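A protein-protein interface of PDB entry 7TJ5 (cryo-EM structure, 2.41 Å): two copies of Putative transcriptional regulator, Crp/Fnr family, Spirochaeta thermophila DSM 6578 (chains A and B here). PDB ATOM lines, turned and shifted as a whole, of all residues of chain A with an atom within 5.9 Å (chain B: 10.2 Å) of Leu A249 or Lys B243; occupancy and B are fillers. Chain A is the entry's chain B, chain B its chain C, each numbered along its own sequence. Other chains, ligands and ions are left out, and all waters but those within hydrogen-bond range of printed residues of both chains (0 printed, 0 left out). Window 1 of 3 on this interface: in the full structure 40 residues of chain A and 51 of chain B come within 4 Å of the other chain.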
ATOM      1  N   VAL A 241     -12.178  -6.145  28.962  1.00  0.00           N
ATOM      2  CA  VAL A 241     -12.401  -7.178  27.956  1.00  0.00           C
ATOM      3  C   VAL A 241     -11.666  -8.472  28.306  1.00  0.00           C
ATOM      4  O   VAL A 241     -12.151  -9.567  27.993  1.00  0.00           O
ATOM      5  CB  VAL A 241     -11.990  -6.632  26.573  1.00  0.00           C
ATOM      6  CG1 VAL A 241     -11.840  -7.745  25.549  1.00  0.00           C
ATOM      7  CG2 VAL A 241     -13.002  -5.602  26.094  1.00  0.00           C
ATOM      8  N   SER A 242     -10.523  -8.383  28.996  1.00  0.00           N
ATOM      9  CA  SER A 242      -9.771  -9.588  29.347  1.00  0.00           C
ATOM     10  C   SER A 242     -10.560 -10.522  30.262  1.00  0.00           C
ATOM     11  O   SER A 242     -10.459 -11.749  30.139  1.00  0.00           O
ATOM     12  CB  SER A 242      -8.446  -9.198  30.002  1.00  0.00           C
ATOM     13  OG  SER A 242      -7.480  -8.844  29.029  1.00  0.00           O
ATOM     14  N   ASP A 245     -14.942 -13.501  29.226  1.00  0.00           N
ATOM     15  CA  ASP A 245     -15.317 -14.907  29.057  1.00  0.00           C
ATOM     16  C   ASP A 245     -14.323 -15.819  29.773  1.00  0.00           C
ATOM     17  O   ASP A 245     -13.603 -16.607  29.156  1.00  0.00           O
ATOM     18  CB  ASP A 245     -15.413 -15.250  27.563  1.00  0.00           C
ATOM     19  CG  ASP A 245     -16.745 -14.853  26.958  1.00  0.00           C
ATOM     20  OD1 ASP A 245     -17.662 -14.488  27.724  1.00  0.00           O
ATOM     21  OD2 ASP A 245     -16.877 -14.909  25.716  1.00  0.00           O
ATOM     22  N   ALA A 246     -14.289 -15.701  31.101  1.00  0.00           N
ATOM     23  CA  ALA A 246     -13.313 -16.443  31.895  1.00  0.00           C
ATOM     24  C   ALA A 246     -13.629 -17.936  31.931  1.00  0.00           C
ATOM     25  O   ALA A 246     -12.743 -18.776  31.718  1.00  0.00           O
ATOM     26  CB  ALA A 246     -13.256 -15.872  33.313  1.00  0.00           C
ATOM     27  N   ALA A 247     -14.891 -18.289  32.201  1.00  0.00           N
ATOM     28  CA  ALA A 247     -15.272 -19.695  32.317  1.00  0.00           C
ATOM     29  C   ALA A 247     -15.169 -20.425  30.983  1.00  0.00           C
ATOM     30  O   ALA A 247     -14.727 -21.581  30.938  1.00  0.00           O
ATOM     31  CB  ALA A 247     -16.687 -19.808  32.881  1.00  0.00           C
ATOM     32  N   LYS A 248     -15.577 -19.776  29.891  1.00  0.00           N
ATOM     33  CA  LYS A 248     -15.467 -20.401  28.578  1.00  0.00           C
ATOM     34  C   LYS A 248     -14.011 -20.664  28.219  1.00  0.00           C
ATOM     35  O   LYS A 248     -13.678 -21.726  27.683  1.00  0.00           O
ATOM     36  CB  LYS A 248     -16.139 -19.532  27.516  1.00  0.00           C
ATOM     37  CG  LYS A 248     -16.473 -20.283  26.235  1.00  0.00           C
ATOM     38  CD  LYS A 248     -17.129 -19.376  25.207  1.00  0.00           C
ATOM     39  CE  LYS A 248     -18.642 -19.446  25.301  1.00  0.00           C
ATOM     40  NZ  LYS A 248     -19.310 -18.807  24.136  1.00  0.00           N
ATOM     41  N   LEU A 249     -13.129 -19.709  28.515  1.00  0.00           N
ATOM     42  CA  LEU A 249     -11.712 -19.899  28.229  1.00  0.00           C
ATOM     43  C   LEU A 249     -11.113 -21.000  29.094  1.00  0.00           C
ATOM     44  O   LEU A 249     -10.308 -21.803  28.610  1.00  0.00           O
ATOM     45  CB  LEU A 249     -10.955 -18.586  28.427  1.00  0.00           C
ATOM     46  CG  LEU A 249     -11.047 -17.600  27.263  1.00  0.00           C
ATOM     47  CD1 LEU A 249     -10.479 -16.249  27.655  1.00  0.00           C
ATOM     48  CD2 LEU A 249     -10.327 -18.153  26.044  1.00  0.00           C
ATOM     49  N   LEU A 250     -11.503 -21.063  30.370  1.00  0.00           N
ATOM     50  CA  LEU A 250     -11.017 -22.133  31.239  1.00  0.00           C
ATOM     51  C   LEU A 250     -11.454 -23.501  30.723  1.00  0.00           C
ATOM     52  O   LEU A 250     -10.650 -24.442  30.663  1.00  0.00           O
ATOM     53  CB  LEU A 250     -11.510 -21.913  32.668  1.00  0.00           C
ATOM     54  CG  LEU A 250     -10.449 -21.511  33.691  1.00  0.00           C
ATOM     55  CD1 LEU A 250     -11.090 -21.272  35.046  1.00  0.00           C
ATOM     56  CD2 LEU A 250      -9.373 -22.578  33.781  1.00  0.00           C
ATOM     57  N   HIS A 251     -12.725 -23.624  30.331  1.00  0.00           N
ATOM     58  CA  HIS A 251     -13.210 -24.889  29.790  1.00  0.00           C
ATOM     59  C   HIS A 251     -12.495 -25.241  28.492  1.00  0.00           C
ATOM     60  O   HIS A 251     -12.143 -26.406  28.263  1.00  0.00           O
ATOM     61  CB  HIS A 251     -14.723 -24.818  29.572  1.00  0.00           C
ATOM     62  CG  HIS A 251     -15.339 -26.118  29.153  1.00  0.00           C
ATOM     63  ND1 HIS A 251     -15.657 -27.112  30.051  1.00  0.00           N
ATOM     64  CD2 HIS A 251     -15.701 -26.581  27.933  1.00  0.00           C
ATOM     65  CE1 HIS A 251     -16.185 -28.135  29.404  1.00  0.00           C
ATOM     66  NE2 HIS A 251     -16.225 -27.838  28.117  1.00  0.00           N
ATOM     67  N   ARG A 252     -12.277 -24.245  27.625  1.00  0.00           N
ATOM     68  CA  ARG A 252     -11.583 -24.489  26.364  1.00  0.00           C
ATOM     69  C   ARG A 252     -10.156 -24.967  26.605  1.00  0.00           C
ATOM     70  O   ARG A 252      -9.684 -25.891  25.931  1.00  0.00           O
ATOM     71  CB  ARG A 252     -11.607 -23.219  25.513  1.00  0.00           C
ATOM     72  CG  ARG A 252     -10.693 -23.235  24.304  1.00  0.00           C
ATOM     73  CD  ARG A 252     -10.825 -21.940  23.517  1.00  0.00           C
ATOM     74  NE  ARG A 252     -10.364 -22.086  22.141  1.00  0.00           N
ATOM     75  CZ  ARG A 252     -11.140 -22.449  21.129  1.00  0.00           C
ATOM     76  NH1 ARG A 252     -12.427 -22.700  21.300  1.00  0.00           N
ATOM     77  NH2 ARG A 252     -10.610 -22.560  19.914  1.00  0.00           N
ATOM     78  N   GLU A 253      -9.474 -24.397  27.604  1.00  0.00           N
ATOM     79  CA  GLU A 253      -8.098 -24.809  27.878  1.00  0.00           C
ATOM     80  C   GLU A 253      -8.061 -26.205  28.482  1.00  0.00           C
ATOM     81  O   GLU A 253      -7.154 -26.991  28.184  1.00  0.00           O
ATOM     82  CB  GLU A 253      -7.386 -23.808  28.791  1.00  0.00           C
ATOM     83  CG  GLU A 253      -6.417 -22.860  28.074  1.00  0.00           C
ATOM     84  CD  GLU A 253      -7.076 -21.662  27.423  1.00  0.00           C
ATOM     85  OE1 GLU A 253      -7.777 -20.911  28.131  1.00  0.00           O
ATOM     86  OE2 GLU A 253      -6.879 -21.465  26.206  1.00  0.00           O
ATOM     87  N   ARG A 254      -9.048 -26.538  29.316  1.00  0.00           N
ATOM     88  CA  ARG A 254      -9.122 -27.888  29.863  1.00  0.00           C
ATOM     89  C   ARG A 254      -9.346 -28.914  28.756  1.00  0.00           C
ATOM     90  O   ARG A 254      -8.688 -29.962  28.722  1.00  0.00           O
ATOM     91  CB  ARG A 254     -10.234 -27.972  30.905  1.00  0.00           C
ATOM     92  CG  ARG A 254     -10.467 -29.373  31.433  1.00  0.00           C
ATOM     93  CD  ARG A 254     -11.337 -29.357  32.668  1.00  0.00           C
ATOM     94  NE  ARG A 254     -12.581 -28.631  32.446  1.00  0.00           N
ATOM     95  CZ  ARG A 254     -13.656 -28.740  33.212  1.00  0.00           C
ATOM     96  NH1 ARG A 254     -13.682 -29.557  34.252  1.00  0.00           N
ATOM     97  NH2 ARG A 254     -14.734 -28.015  32.927  1.00  0.00           N
ATOM     98  N   GLU A 256      -8.586 -28.574  25.578  1.00  0.00           N
ATOM     99  CA  GLU A 256      -7.385 -28.647  24.747  1.00  0.00           C
ATOM    100  C   GLU A 256      -6.298 -29.477  25.418  1.00  0.00           C
ATOM    101  O   GLU A 256      -5.654 -30.311  24.769  1.00  0.00           O
ATOM    102  CB  GLU A 256      -6.870 -27.250  24.392  1.00  0.00           C
ATOM    103  CG  GLU A 256      -7.801 -26.451  23.487  1.00  0.00           C
ATOM    104  CD  GLU A 256      -7.643 -24.950  23.648  1.00  0.00           C
ATOM    105  OE1 GLU A 256      -7.415 -24.486  24.782  1.00  0.00           O
ATOM    106  OE2 GLU A 256      -7.749 -24.230  22.632  1.00  0.00           O
ATOM    107  N   SER B 146     -19.625 -20.725  18.789  1.00  0.00           N
ATOM    108  CA  SER B 146     -18.926 -20.574  20.059  1.00  0.00           C
ATOM    109  C   SER B 146     -17.938 -21.696  20.347  1.00  0.00           C
ATOM    110  O   SER B 146     -17.105 -21.536  21.245  1.00  0.00           O
ATOM    111  CB  SER B 146     -19.939 -20.481  21.201  1.00  0.00           C
ATOM    112  OG  SER B 146     -21.001 -21.402  21.017  1.00  0.00           O
ATOM    113  N   ILE B 149     -14.604 -21.696  16.968  1.00  0.00           N
ATOM    114  CA  ILE B 149     -13.759 -20.514  16.885  1.00  0.00           C
ATOM    115  C   ILE B 149     -13.463 -20.020  18.296  1.00  0.00           C
ATOM    116  O   ILE B 149     -14.312 -20.120  19.189  1.00  0.00           O
ATOM    117  CB  ILE B 149     -14.437 -19.415  16.040  1.00  0.00           C
ATOM    118  CG1 ILE B 149     -14.880 -19.974  14.688  1.00  0.00           C
ATOM    119  CG2 ILE B 149     -13.499 -18.240  15.806  1.00  0.00           C
ATOM    120  CD1 ILE B 149     -13.762 -20.594  13.874  1.00  0.00           C
ATOM    121  N   ASN B 150     -12.252 -19.506  18.494  1.00  0.00           N
ATOM    122  CA  ASN B 150     -11.892 -18.859  19.748  1.00  0.00           C
ATOM    123  C   ASN B 150     -12.835 -17.682  19.980  1.00  0.00           C
ATOM    124  O   ASN B 150     -12.986 -16.836  19.090  1.00  0.00           O
ATOM    125  CB  ASN B 150     -10.435 -18.388  19.674  1.00  0.00           C
ATOM    126  CG  ASN B 150      -9.908 -17.815  20.987  1.00  0.00           C
ATOM    127  OD1 ASN B 150     -10.655 -17.532  21.920  1.00  0.00           O
ATOM    128  ND2 ASN B 150      -8.595 -17.646  21.056  1.00  0.00           N
ATOM    129  N   PRO B 151     -13.501 -17.602  21.139  1.00  0.00           N
ATOM    130  CA  PRO B 151     -14.469 -16.512  21.354  1.00  0.00           C
ATOM    131  C   PRO B 151     -13.865 -15.119  21.268  1.00  0.00           C
ATOM    132  O   PRO B 151     -14.556 -14.190  20.830  1.00  0.00           O
ATOM    133  CB  PRO B 151     -15.026 -16.806  22.757  1.00  0.00           C
ATOM    134  CG  PRO B 151     -14.105 -17.826  23.357  1.00  0.00           C
ATOM    135  CD  PRO B 151     -13.567 -18.611  22.209  1.00  0.00           C
ATOM    136  N   ALA B 152     -12.607 -14.939  21.676  1.00  0.00           N
ATOM    137  CA  ALA B 152     -11.966 -13.634  21.523  1.00  0.00           C
ATOM    138  C   ALA B 152     -11.828 -13.256  20.054  1.00  0.00           C
ATOM    139  O   ALA B 152     -12.073 -12.104  19.675  1.00  0.00           O
ATOM    140  CB  ALA B 152     -10.602 -13.632  22.212  1.00  0.00           C
ATOM    141  N   LEU B 153     -11.433 -14.214  19.211  1.00  0.00           N
ATOM    142  CA  LEU B 153     -11.330 -13.950  17.779  1.00  0.00           C
ATOM    143  C   LEU B 153     -12.692 -13.640  17.171  1.00  0.00           C
ATOM    144  O   LEU B 153     -12.809 -12.759  16.310  1.00  0.00           O
ATOM    145  CB  LEU B 153     -10.681 -15.140  17.074  1.00  0.00           C
ATOM    146  CG  LEU B 153     -10.341 -14.926  15.599  1.00  0.00           C
ATOM    147  CD1 LEU B 153      -9.249 -13.879  15.453  1.00  0.00           C
ATOM    148  CD2 LEU B 153      -9.923 -16.232  14.946  1.00  0.00           C
ATOM    149  N   LEU B 154     -13.735 -14.351  17.608  1.00  0.00           N
ATOM    150  CA  LEU B 154     -15.078 -14.077  17.104  1.00  0.00           C
ATOM    151  C   LEU B 154     -15.533 -12.683  17.511  1.00  0.00           C
ATOM    152  O   LEU B 154     -16.153 -11.964  16.717  1.00  0.00           O
ATOM    153  CB  LEU B 154     -16.057 -15.132  17.613  1.00  0.00           C
ATOM    154  CG  LEU B 154     -17.227 -15.470  16.687  1.00  0.00           C
ATOM    155  CD1 LEU B 154     -16.797 -16.453  15.612  1.00  0.00           C
ATOM    156  CD2 LEU B 154     -18.399 -16.017  17.486  1.00  0.00           C
ATOM    157  N   ARG B 155     -15.226 -12.286  18.747  1.00  0.00           N
ATOM    158  CA  ARG B 155     -15.578 -10.951  19.217  1.00  0.00           C
ATOM    159  C   ARG B 155     -14.850  -9.888  18.408  1.00  0.00           C
ATOM    160  O   ARG B 155     -15.444  -8.876  18.020  1.00  0.00           O
ATOM    161  CB  ARG B 155     -15.240 -10.834  20.702  1.00  0.00           C
ATOM    162  CG  ARG B 155     -15.775  -9.607  21.399  1.00  0.00           C
ATOM    163  CD  ARG B 155     -15.385  -9.660  22.863  1.00  0.00           C
ATOM    164  NE  ARG B 155     -16.397 -10.335  23.665  1.00  0.00           N
ATOM    165  CZ  ARG B 155     -16.166 -10.883  24.849  1.00  0.00           C
ATOM    166  NH1 ARG B 155     -14.963 -10.858  25.400  1.00  0.00           N
ATOM    167  NH2 ARG B 155     -17.165 -11.477  25.497  1.00  0.00           N
ATOM    168  N   GLY B 235      -8.040  -3.098  22.958  1.00  0.00           N
ATOM    169  CA  GLY B 235      -8.296  -3.996  24.073  1.00  0.00           C
ATOM    170  C   GLY B 235      -8.568  -5.422  23.633  1.00  0.00           C
ATOM    171  O   GLY B 235      -8.078  -6.375  24.246  1.00  0.00           O
ATOM    172  N   ASN B 236      -9.344  -5.586  22.557  1.00  0.00           N
ATOM    173  CA  ASN B 236      -9.593  -6.920  22.015  1.00  0.00           C
ATOM    174  C   ASN B 236      -8.303  -7.581  21.549  1.00  0.00           C
ATOM    175  O   ASN B 236      -8.080  -8.769  21.805  1.00  0.00           O
ATOM    176  CB  ASN B 236     -10.598  -6.845  20.863  1.00  0.00           C
ATOM    177  CG  ASN B 236     -12.036  -6.876  21.339  1.00  0.00           C
ATOM    178  OD1 ASN B 236     -12.306  -6.940  22.534  1.00  0.00           O
ATOM    179  ND2 ASN B 236     -12.969  -6.844  20.396  1.00  0.00           N
ATOM    180  N   ILE B 237      -7.442  -6.826  20.861  1.00  0.00           N
ATOM    181  CA  ILE B 237      -6.186  -7.391  20.374  1.00  0.00           C
ATOM    182  C   ILE B 237      -5.280  -7.779  21.539  1.00  0.00           C
ATOM    183  O   ILE B 237      -4.656  -8.850  21.529  1.00  0.00           O
ATOM    184  CB  ILE B 237      -5.494  -6.403  19.417  1.00  0.00           C
ATOM    185  CG1 ILE B 237      -6.275  -6.299  18.106  1.00  0.00           C
ATOM    186  CG2 ILE B 237      -4.061  -6.829  19.141  1.00  0.00           C
ATOM    187  CD1 ILE B 237      -5.751  -5.237  17.170  1.00  0.00           C
ATOM    188  N   ALA B 238      -5.199  -6.926  22.565  1.00  0.00           N
ATOM    189  CA  ALA B 238      -4.371  -7.238  23.725  1.00  0.00           C
ATOM    190  C   ALA B 238      -4.882  -8.473  24.455  1.00  0.00           C
ATOM    191  O   ALA B 238      -4.091  -9.324  24.883  1.00  0.00           O
ATOM    192  CB  ALA B 238      -4.318  -6.039  24.670  1.00  0.00           C
ATOM    193  N   SER B 239      -6.206  -8.599  24.592  1.00  0.00           N
ATOM    194  CA  SER B 239      -6.775  -9.788  25.217  1.00  0.00           C
ATOM    195  C   SER B 239      -6.490 -11.034  24.388  1.00  0.00           C
ATOM    196  O   SER B 239      -6.165 -12.090  24.938  1.00  0.00           O
ATOM    197  CB  SER B 239      -8.279  -9.606  25.416  1.00  0.00           C
ATOM    198  OG  SER B 239      -8.891 -10.817  25.824  1.00  0.00           O
ATOM    199  N   LEU B 240      -6.601 -10.927  23.061  1.00  0.00           N
ATOM    200  CA  LEU B 240      -6.341 -12.077  22.201  1.00  0.00           C
ATOM    201  C   LEU B 240      -4.885 -12.514  22.296  1.00  0.00           C
ATOM    202  O   LEU B 240      -4.583 -13.712  22.269  1.00  0.00           O
ATOM    203  CB  LEU B 240      -6.704 -11.742  20.755  1.00  0.00           C
ATOM    204  CG  LEU B 240      -6.821 -12.909  19.773  1.00  0.00           C
ATOM    205  CD1 LEU B 240      -8.039 -12.728  18.888  1.00  0.00           C
ATOM    206  CD2 LEU B 240      -5.564 -13.041  18.928  1.00  0.00           C
ATOM    207  N   VAL B 241      -3.968 -11.553  22.409  1.00  0.00           N
ATOM    208  CA  VAL B 241      -2.548 -11.885  22.391  1.00  0.00           C
ATOM    209  C   VAL B 241      -2.069 -12.381  23.756  1.00  0.00           C
ATOM    210  O   VAL B 241      -1.173 -13.233  23.829  1.00  0.00           O
ATOM    211  CB  VAL B 241      -1.750 -10.657  21.907  1.00  0.00           C
ATOM    212  CG1 VAL B 241      -0.266 -10.793  22.213  1.00  0.00           C
ATOM    213  CG2 VAL B 241      -1.969 -10.444  20.416  1.00  0.00           C
ATOM    214  N   SER B 242      -2.679 -11.909  24.849  1.00  0.00           N
ATOM    215  CA  SER B 242      -2.253 -12.339  26.182  1.00  0.00           C
ATOM    216  C   SER B 242      -2.446 -13.839  26.399  1.00  0.00           C
ATOM    217  O   SER B 242      -1.624 -14.484  27.063  1.00  0.00           O
ATOM    218  CB  SER B 242      -3.010 -11.549  27.247  1.00  0.00           C
ATOM    219  OG  SER B 242      -2.431 -10.270  27.443  1.00  0.00           O
ATOM    220  N   LYS B 243      -3.514 -14.415  25.853  1.00  0.00           N
ATOM    221  CA  LYS B 243      -3.855 -15.815  26.083  1.00  0.00           C
ATOM    222  C   LYS B 243      -3.303 -16.762  25.019  1.00  0.00           C
ATOM    223  O   LYS B 243      -3.750 -17.912  24.949  1.00  0.00           O
ATOM    224  CB  LYS B 243      -5.374 -15.983  26.178  1.00  0.00           C
ATOM    225  CG  LYS B 243      -6.020 -15.173  27.289  1.00  0.00           C
ATOM    226  CD  LYS B 243      -7.228 -14.404  26.784  1.00  0.00           C
ATOM    227  CE  LYS B 243      -7.834 -13.541  27.879  1.00  0.00           C
ATOM    228  NZ  LYS B 243      -6.819 -13.120  28.883  1.00  0.00           N
ATOM    229  N   LEU B 244      -2.359 -16.317  24.190  1.00  0.00           N
ATOM    230  CA  LEU B 244      -1.885 -17.153  23.091  1.00  0.00           C
ATOM    231  C   LEU B 244      -1.015 -18.315  23.575  1.00  0.00           C
ATOM    232  O   LEU B 244      -1.387 -19.483  23.416  1.00  0.00           O
ATOM    233  CB  LEU B 244      -1.136 -16.296  22.067  1.00  0.00           C
ATOM    234  CG  LEU B 244      -2.043 -15.696  20.985  1.00  0.00           C
ATOM    235  CD1 LEU B 244      -1.236 -15.070  19.861  1.00  0.00           C
ATOM    236  CD2 LEU B 244      -3.001 -16.745  20.435  1.00  0.00           C
ATOM    237  N   ASP B 245       0.138 -18.023  24.169  1.00  0.00           N
ATOM    238  CA  ASP B 245       1.101 -19.063  24.542  1.00  0.00           C
ATOM    239  C   ASP B 245       1.059 -19.321  26.047  1.00  0.00           C
ATOM    240  O   ASP B 245       2.021 -19.074  26.776  1.00  0.00           O
ATOM    241  CB  ASP B 245       2.511 -18.662  24.084  1.00  0.00           C
ATOM    242  CG  ASP B 245       2.766 -18.990  22.627  1.00  0.00           C
ATOM    243  OD1 ASP B 245       1.930 -19.693  22.020  1.00  0.00           O
ATOM    244  OD2 ASP B 245       3.802 -18.548  22.087  1.00  0.00           O
ATOM    245  N   ALA B 246      -0.086 -19.826  26.511  1.00  0.00           N
ATOM    246  CA  ALA B 246      -0.291 -20.025  27.944  1.00  0.00           C
ATOM    247  C   ALA B 246       0.558 -21.174  28.484  1.00  0.00           C
ATOM    248  O   ALA B 246       1.225 -21.036  29.518  1.00  0.00           O
ATOM    249  CB  ALA B 246      -1.773 -20.273  28.226  1.00  0.00           C
ATOM    250  N   ALA B 247       0.545 -22.320  27.795  1.00  0.00           N
ATOM    251  CA  ALA B 247       1.278 -23.492  28.269  1.00  0.00           C
ATOM    252  C   ALA B 247       2.786 -23.280  28.224  1.00  0.00           C
ATOM    253  O   ALA B 247       3.502 -23.699  29.143  1.00  0.00           O
ATOM    254  CB  ALA B 247       0.886 -24.721  27.449  1.00  0.00           C
ATOM    255  N   LYS B 248       3.288 -22.642  27.165  1.00  0.00           N
ATOM    256  CA  LYS B 248       4.718 -22.368  27.079  1.00  0.00           C
ATOM    257  C   LYS B 248       5.165 -21.441  28.200  1.00  0.00           C
ATOM    258  O   LYS B 248       6.222 -21.648  28.803  1.00  0.00           O
ATOM    259  CB  LYS B 248       5.065 -21.774  25.714  1.00  0.00           C
ATOM    260  CG  LYS B 248       6.542 -21.876  25.364  1.00  0.00           C
ATOM    261  CD  LYS B 248       6.840 -21.264  24.005  1.00  0.00           C
ATOM    262  CE  LYS B 248       6.804 -22.315  22.911  1.00  0.00           C
ATOM    263  NZ  LYS B 248       7.370 -21.817  21.628  1.00  0.00           N
ATOM    264  N   LEU B 249       4.364 -20.417  28.500  1.00  0.00           N
ATOM    265  CA  LEU B 249       4.710 -19.501  29.581  1.00  0.00           C
ATOM    266  C   LEU B 249       4.657 -20.197  30.935  1.00  0.00           C
ATOM    267  O   LEU B 249       5.522 -19.967  31.787  1.00  0.00           O
ATOM    268  CB  LEU B 249       3.779 -18.290  29.561  1.00  0.00           C
ATOM    269  CG  LEU B 249       4.141 -17.207  28.545  1.00  0.00           C
ATOM    270  CD1 LEU B 249       3.030 -16.181  28.434  1.00  0.00           C
ATOM    271  CD2 LEU B 249       5.453 -16.543  28.927  1.00  0.00           C
ATOM    272  N   LEU B 250       3.661 -21.063  31.147  1.00  0.00           N
ATOM    273  CA  LEU B 250       3.588 -21.812  32.399  1.00  0.00           C
ATOM    274  C   LEU B 250       4.809 -22.711  32.573  1.00  0.00           C
ATOM    275  O   LEU B 250       5.411 -22.759  33.656  1.00  0.00           O
ATOM    276  CB  LEU B 250       2.302 -22.636  32.442  1.00  0.00           C
ATOM    277  CG  LEU B 250       1.239 -22.171  33.437  1.00  0.00           C
ATOM    278  CD1 LEU B 250       0.002 -23.043  33.328  1.00  0.00           C
ATOM    279  CD2 LEU B 250       1.795 -22.191  34.849  1.00  0.00           C
ATOM    280  N   ARG B 287       3.893 -31.195  26.281  1.00  0.00           N
ATOM    281  CA  ARG B 287       3.745 -29.752  26.481  1.00  0.00           C
ATOM    282  C   ARG B 287       3.787 -29.372  27.959  1.00  0.00           C
ATOM    283  O   ARG B 287       3.123 -28.425  28.388  1.00  0.00           O
ATOM    284  CB  ARG B 287       2.467 -29.224  25.820  1.00  0.00           C
ATOM    285  CG  ARG B 287       2.601 -29.017  24.318  1.00  0.00           C
ATOM    286  CD  ARG B 287       1.253 -28.812  23.651  1.00  0.00           C
ATOM    287  NE  ARG B 287       0.549 -27.660  24.201  1.00  0.00           N
ATOM    288  CZ  ARG B 287       0.564 -26.449  23.664  1.00  0.00           C
ATOM    289  NH1 ARG B 287       1.248 -26.191  22.562  1.00  0.00           N
ATOM    290  NH2 ARG B 287      -0.117 -25.469  24.252  1.00  0.00           N
ATOM    291  N   TYR B 289       2.881 -31.226  30.772  1.00  0.00           N
ATOM    292  CA  TYR B 289       1.684 -31.600  31.510  1.00  0.00           C
ATOM    293  C   TYR B 289       1.908 -32.899  32.271  1.00  0.00           C
ATOM    294  O   TYR B 289       2.382 -33.886  31.699  1.00  0.00           O
ATOM    295  CB  TYR B 289       0.481 -31.755  30.575  1.00  0.00           C
ATOM    296  CG  TYR B 289      -0.039 -30.461  29.993  1.00  0.00           C
ATOM    297  CD1 TYR B 289      -0.087 -29.303  30.759  1.00  0.00           C
ATOM    298  CD2 TYR B 289      -0.501 -30.402  28.686  1.00  0.00           C
ATOM    299  CE1 TYR B 289      -0.566 -28.119  30.232  1.00  0.00           C
ATOM    300  CE2 TYR B 289      -0.983 -29.225  28.151  1.00  0.00           C
ATOM    301  CZ  TYR B 289      -1.013 -28.086  28.928  1.00  0.00           C
ATOM    302  OH  TYR B 289      -1.498 -26.912  28.401  1.00  0.00           O
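The guanidinium group (NH2) of Arg B155 lies within salt-bridge range of the side-chain carboxylate (OD2) of Asp A245 (3.5 Å).
The backbone carbonyl oxygen of Leu A249 sits close to the side-chain carboxylate of Glu A253 (2.7 Å).
OE2 of Glu A256 is in salt-bridge range of NE of Arg A252 (3.4 Å).
The side-chain amide oxygen (OD1) of Asn B150 sits close to the backbone NH (N) of Ala B152.
CG1 of Val A241 touches OD1 of Asn B236, at 3.2 Å.
Ser A242 touches Ser B239.
Ser A242 touches Lys B243 (O to CE, 3.9 Å).
OD2 of Asp A245 touches CB of Pro B151, 3.97 Å away.
Lys A248 touches Ser B146.
Lys A248 touches Pro B151.
Leu A249 touches Lys B243 (CD1 to CE, 3.8 Å).
O of Ile B149 touches NH1 of Arg A252, 3.8 Å away.
Arg A252 touches Asn B150.
Leu A249 touches just one residue of chain B: Lys B243 (3.8 Å).
Lys B243 touches just these residues of chain A: Ser A242 and Leu A249.
Of chain B, only Ser B239 and Lys B243 come within 4 Å of Ser A242.
No residue of chain B comes within 4 Å of Ala A247.
No residue of chain B comes within 4 Å of Leu A250.
Of the printed residues of chain B, Asp A245 touches Pro B151 and Arg B155.
Of the printed residues of chain A, Ser B146 touches Lys A248.
Printed residues of chain A within 4 Å of Ile B149: Arg A252.
Of the printed residues of chain A, Arg B155 touches Asp A245 (3.5 Å).
Printed residues of chain A within 4 Å of Ser B239: Ser A242 (3.8 Å).
The nearest residue of chain B that does not touch Leu A249 is Asn B150 (4.2 Å).
Of the 13 printed residues of chain A, 6 touch a printed residue of chain B.
Hydrophobic or aromatic side chains of chain A that line the printed part of chain B: Val A241 and Leu A249.
Among the printed residues, 10 pairs touch across the chains.
Positions printed for both chains: 241, 242, 245, 246, 247, 248, 249 and 250.
Of the 10 pairs that touch across the chains among the printed residues, none has its exchanged pair printed and touching as well.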
